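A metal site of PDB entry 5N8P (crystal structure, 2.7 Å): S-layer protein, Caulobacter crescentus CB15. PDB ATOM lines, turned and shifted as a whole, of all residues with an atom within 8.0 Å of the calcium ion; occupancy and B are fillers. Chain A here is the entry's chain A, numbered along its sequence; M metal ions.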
ATOM      1  N   LEU A 962      24.685   4.695 -16.469  1.00  0.00           N
ATOM      2  CA  LEU A 962      25.854   5.571 -16.286  1.00  0.00           C
ATOM      3  C   LEU A 962      25.456   6.851 -15.572  1.00  0.00           C
ATOM      4  O   LEU A 962      25.964   7.145 -14.477  1.00  0.00           O
ATOM      5  CB  LEU A 962      26.565   5.887 -17.621  1.00  0.00           C
ATOM      6  CG  LEU A 962      27.388   4.763 -18.291  1.00  0.00           C
ATOM      7  CD1 LEU A 962      27.557   5.051 -19.783  1.00  0.00           C
ATOM      8  CD2 LEU A 962      28.738   4.577 -17.603  1.00  0.00           C
ATOM      9  N   ASP A 963      24.512   7.582 -16.178  1.00  0.00           N
ATOM     10  CA  ASP A 963      23.887   8.772 -15.597  1.00  0.00           C
ATOM     11  C   ASP A 963      23.411   8.553 -14.146  1.00  0.00           C
ATOM     12  O   ASP A 963      23.671   9.395 -13.250  1.00  0.00           O
ATOM     13  CB  ASP A 963      22.742   9.273 -16.475  1.00  0.00           C
ATOM     14  CG  ASP A 963      23.221  10.014 -17.731  1.00  0.00           C
ATOM     15  OD1 ASP A 963      24.242  10.741 -17.679  1.00  0.00           O
ATOM     16  OD2 ASP A 963      22.561   9.855 -18.774  1.00  0.00           O
ATOM     17  N   ALA A 964      22.748   7.406 -13.906  1.00  0.00           N
ATOM     18  CA  ALA A 964      22.311   7.028 -12.558  1.00  0.00           C
ATOM     19  C   ALA A 964      23.502   6.926 -11.594  1.00  0.00           C
ATOM     20  O   ALA A 964      23.457   7.483 -10.511  1.00  0.00           O
ATOM     21  CB  ALA A 964      21.487   5.736 -12.595  1.00  0.00           C
ATOM     22  N   ALA A 965      24.570   6.249 -12.040  1.00  0.00           N
ATOM     23  CA  ALA A 965      25.779   5.996 -11.235  1.00  0.00           C
ATOM     24  C   ALA A 965      26.531   7.283 -10.903  1.00  0.00           C
ATOM     25  O   ALA A 965      27.116   7.392  -9.821  1.00  0.00           O
ATOM     26  CB  ALA A 965      26.686   4.995 -11.933  1.00  0.00           C
ATOM     27  N   ALA A 966      26.502   8.235 -11.816  1.00  0.00           N
ATOM     28  CA  ALA A 966      27.227   9.493 -11.626  1.00  0.00           C
ATOM     29  C   ALA A 966      26.346  10.589 -11.066  1.00  0.00           C
ATOM     30  O   ALA A 966      26.748  11.761 -11.080  1.00  0.00           O
ATOM     31  CB  ALA A 966      27.829   9.939 -12.939  1.00  0.00           C
ATOM     32  N   ALA A 967      25.153  10.234 -10.571  1.00  0.00           N
ATOM     33  CA  ALA A 967      24.174  11.235 -10.107  1.00  0.00           C
ATOM     34  C   ALA A 967      24.726  12.216  -9.062  1.00  0.00           C
ATOM     35  O   ALA A 967      24.456  13.421  -9.153  1.00  0.00           O
ATOM     36  CB  ALA A 967      22.876  10.580  -9.628  1.00  0.00           C
ATOM     37  N   GLY A 968      25.518  11.687  -8.120  1.00  0.00           N
ATOM     38  CA  GLY A 968      26.095  12.443  -7.010  1.00  0.00           C
ATOM     39  C   GLY A 968      27.072  13.556  -7.381  1.00  0.00           C
ATOM     40  O   GLY A 968      27.335  13.818  -8.566  1.00  0.00           O
ATOM     41  N   ASP A 969      27.607  14.200  -6.348  1.00  0.00           N
ATOM     42  CA  ASP A 969      28.584  15.280  -6.532  1.00  0.00           C
ATOM     43  C   ASP A 969      30.039  14.838  -6.284  1.00  0.00           C
ATOM     44  O   ASP A 969      30.424  14.537  -5.143  1.00  0.00           O
ATOM     45  CB  ASP A 969      28.238  16.487  -5.656  1.00  0.00           C
ATOM     46  CG  ASP A 969      29.057  17.719  -6.034  1.00  0.00           C
ATOM     47  OD1 ASP A 969      29.445  18.472  -5.112  1.00  0.00           O
ATOM     48  OD2 ASP A 969      29.311  17.927  -7.245  1.00  0.00           O
ATOM     49  N   GLY A 970      30.814  14.837  -7.371  1.00  0.00           N
ATOM     50  CA  GLY A 970      32.235  14.467  -7.335  1.00  0.00           C
ATOM     51  C   GLY A 970      33.216  15.612  -7.468  1.00  0.00           C
ATOM     52  O   GLY A 970      34.398  15.378  -7.730  1.00  0.00           O
ATOM     53  N   SER A 971      32.731  16.841  -7.276  1.00  0.00           N
ATOM     54  CA  SER A 971      33.511  18.081  -7.445  1.00  0.00           C
ATOM     55  C   SER A 971      34.623  18.251  -6.414  1.00  0.00           C
ATOM     56  O   SER A 971      35.714  18.730  -6.757  1.00  0.00           O
ATOM     57  CB  SER A 971      32.600  19.305  -7.404  1.00  0.00           C
ATOM     58  OG  SER A 971      31.816  19.380  -8.569  1.00  0.00           O
ATOM     59  N   VAL A 989      33.701   6.062 -11.764  1.00  0.00           N
ATOM     60  CA  VAL A 989      34.237   7.114 -10.887  1.00  0.00           C
ATOM     61  C   VAL A 989      33.562   8.425 -11.275  1.00  0.00           C
ATOM     62  O   VAL A 989      33.685   8.888 -12.412  1.00  0.00           O
ATOM     63  CB  VAL A 989      35.799   7.234 -10.919  1.00  0.00           C
ATOM     64  CG1 VAL A 989      36.295   8.427 -10.112  1.00  0.00           C
ATOM     65  CG2 VAL A 989      36.463   5.965 -10.402  1.00  0.00           C
ATOM     66  N   ASP A 990      32.828   8.992 -10.309  1.00  0.00           N
ATOM     67  CA  ASP A 990      32.167  10.269 -10.514  1.00  0.00           C
ATOM     68  C   ASP A 990      33.078  11.354  -9.974  1.00  0.00           C
ATOM     69  O   ASP A 990      33.431  11.355  -8.776  1.00  0.00           O
ATOM     70  CB  ASP A 990      30.798  10.297  -9.823  1.00  0.00           C
ATOM     71  CG  ASP A 990      29.959  11.525 -10.169  1.00  0.00           C
ATOM     72  OD1 ASP A 990      30.394  12.399 -10.958  1.00  0.00           O
ATOM     73  OD2 ASP A 990      28.837  11.632  -9.634  1.00  0.00           O
ATOM     74  N   SER A 991      33.481  12.242 -10.878  1.00  0.00           N
ATOM     75  CA  SER A 991      34.311  13.377 -10.534  1.00  0.00           C
ATOM     76  C   SER A 991      33.622  14.701 -10.899  1.00  0.00           C
ATOM     77  O   SER A 991      34.265  15.746 -10.988  1.00  0.00           O
ATOM     78  CB  SER A 991      35.693  13.245 -11.201  1.00  0.00           C
ATOM     79  OG  SER A 991      36.423  12.143 -10.681  1.00  0.00           O
ATOM     80  N   SER A 992      32.286  14.657 -11.058  1.00  0.00           N
ATOM     81  CA  SER A 992      31.526  15.807 -11.574  1.00  0.00           C
ATOM     82  C   SER A 992      30.311  16.265 -10.732  1.00  0.00           C
ATOM     83  O   SER A 992      29.833  15.547  -9.832  1.00  0.00           O
ATOM     84  CB  SER A 992      31.121  15.536 -13.034  1.00  0.00           C
ATOM     85  OG  SER A 992      32.259  15.320 -13.841  1.00  0.00           O
ATOM     86  N   ALA A 993      29.848  17.477 -11.055  1.00  0.00           N
ATOM     87  CA  ALA A 993      28.645  18.091 -10.477  1.00  0.00           C
ATOM     88  C   ALA A 993      27.376  17.290 -10.808  1.00  0.00           C
ATOM     89  O   ALA A 993      27.006  16.376 -10.051  1.00  0.00           O
ATOM     90  CB  ALA A 993      28.523  19.548 -10.938  1.00  0.00           C
ATOM     91  N   GLY A 994      26.748  17.614 -11.963  1.00  0.00           N
ATOM     92  CA  GLY A 994      25.428  17.122 -12.362  1.00  0.00           C
ATOM     93  C   GLY A 994      25.263  15.618 -12.482  1.00  0.00           C
ATOM     94  O   GLY A 994      26.235  14.878 -12.433  1.00  0.00           O
ATOM     95  N   ALA A 995      24.015  15.168 -12.641  1.00  0.00           N
ATOM     96  CA  ALA A 995      23.703  13.750 -12.798  1.00  0.00           C
ATOM     97  C   ALA A 995      23.985  13.214 -14.218  1.00  0.00           C
ATOM     98  O   ALA A 995      23.587  12.083 -14.552  1.00  0.00           O
ATOM     99  CB  ALA A 995      22.267  13.447 -12.353  1.00  0.00           C
ATOM    100  N   THR A 996      24.667  13.997 -15.065  1.00  0.00           N
ATOM    101  CA  THR A 996      25.211  13.469 -16.307  1.00  0.00           C
ATOM    102  C   THR A 996      26.587  12.864 -16.020  1.00  0.00           C
ATOM    103  O   THR A 996      27.457  13.486 -15.387  1.00  0.00           O
ATOM    104  CB  THR A 996      25.306  14.534 -17.432  1.00  0.00           C
ATOM    105  OG1 THR A 996      24.054  15.202 -17.540  1.00  0.00           O
ATOM    106  CG2 THR A 996      25.645  13.905 -18.814  1.00  0.00           C
ATOM    107  N   PHE A 997      26.752  11.613 -16.458  1.00  0.00           N
ATOM    108  CA  PHE A 997      28.065  11.025 -16.631  1.00  0.00           C
ATOM    109  C   PHE A 997      28.709  11.834 -17.757  1.00  0.00           C
ATOM    110  O   PHE A 997      28.235  11.760 -18.901  1.00  0.00           O
ATOM    111  CB  PHE A 997      27.908   9.560 -17.051  1.00  0.00           C
ATOM    112  CG  PHE A 997      29.227   8.838 -17.180  1.00  0.00           C
ATOM    113  CD1 PHE A 997      29.601   7.900 -16.225  1.00  0.00           C
ATOM    114  CD2 PHE A 997      30.092   9.094 -18.251  1.00  0.00           C
ATOM    115  CE1 PHE A 997      30.811   7.241 -16.334  1.00  0.00           C
ATOM    116  CE2 PHE A 997      31.302   8.435 -18.361  1.00  0.00           C
ATOM    117  CZ  PHE A 997      31.663   7.497 -17.400  1.00  0.00           C
ATOM    118  N   VAL A 998      29.732  12.622 -17.432  1.00  0.00           N
ATOM    119  CA  VAL A 998      30.433  13.370 -18.495  1.00  0.00           C
ATOM    120  C   VAL A 998      31.645  12.598 -19.026  1.00  0.00           C
ATOM    121  O   VAL A 998      32.546  12.254 -18.253  1.00  0.00           O
ATOM    122  CB  VAL A 998      30.763  14.858 -18.136  1.00  0.00           C
ATOM    123  CG1 VAL A 998      29.511  15.732 -18.209  1.00  0.00           C
ATOM    124  CG2 VAL A 998      31.464  14.999 -16.784  1.00  0.00           C
ATOM    125  N   ASP A1002      34.475  11.900 -15.876  1.00  0.00           N
ATOM    126  CA  ASP A1002      33.911  10.706 -15.241  1.00  0.00           C
ATOM    127  C   ASP A1002      34.395   9.468 -16.003  1.00  0.00           C
ATOM    128  O   ASP A1002      34.616   9.522 -17.231  1.00  0.00           O
ATOM    129  CB  ASP A1002      32.363  10.732 -15.239  1.00  0.00           C
ATOM    130  CG  ASP A1002      31.794  11.914 -14.446  1.00  0.00           C
ATOM    131  OD1 ASP A1002      32.397  12.341 -13.430  1.00  0.00           O
ATOM    132  OD2 ASP A1002      30.685  12.378 -14.836  1.00  0.00           O
HETATM  133 CA    CA M   1      28.108  13.648 -11.373  1.00  0.00          CA
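N of Ser 992 sits close to OD1 of Asp 990. The side-chain carboxylate (OD1) of Asp 1002 is in hydrogen-bond range of the side-chain hydroxyl (OG) of Ser 992 (3.0 Å). N of Gly 970 lies within hydrogen-bond range of O of Ser 992 (2.7 Å).
O of Ala 966 is bound to the calcium ion, 2.3 Å away. O of Gly 994 is bound to the calcium ion. OD1 of Asp 990 is bound to the calcium ion, at 2.6 Å. The side-chain carboxylate (OD2) of Asp 990 is bound to the calcium ion (2.8 Å). Slightly farther from the calcium ion lies the backbone carbonyl oxygen (O) of Gly 968 (2.9 Å). Slightly farther from the calcium ion lies the backbone carbonyl oxygen (O) of Ser 992 (3.0 Å).
O of Ala 993 touches the calcium ion, 3.2 Å away. Of the 21 residues printed, 6 come within 4 Å of the calcium ion. The nearest printed residue that does not touch the calcium ion is Thr 996 (4.1 Å).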
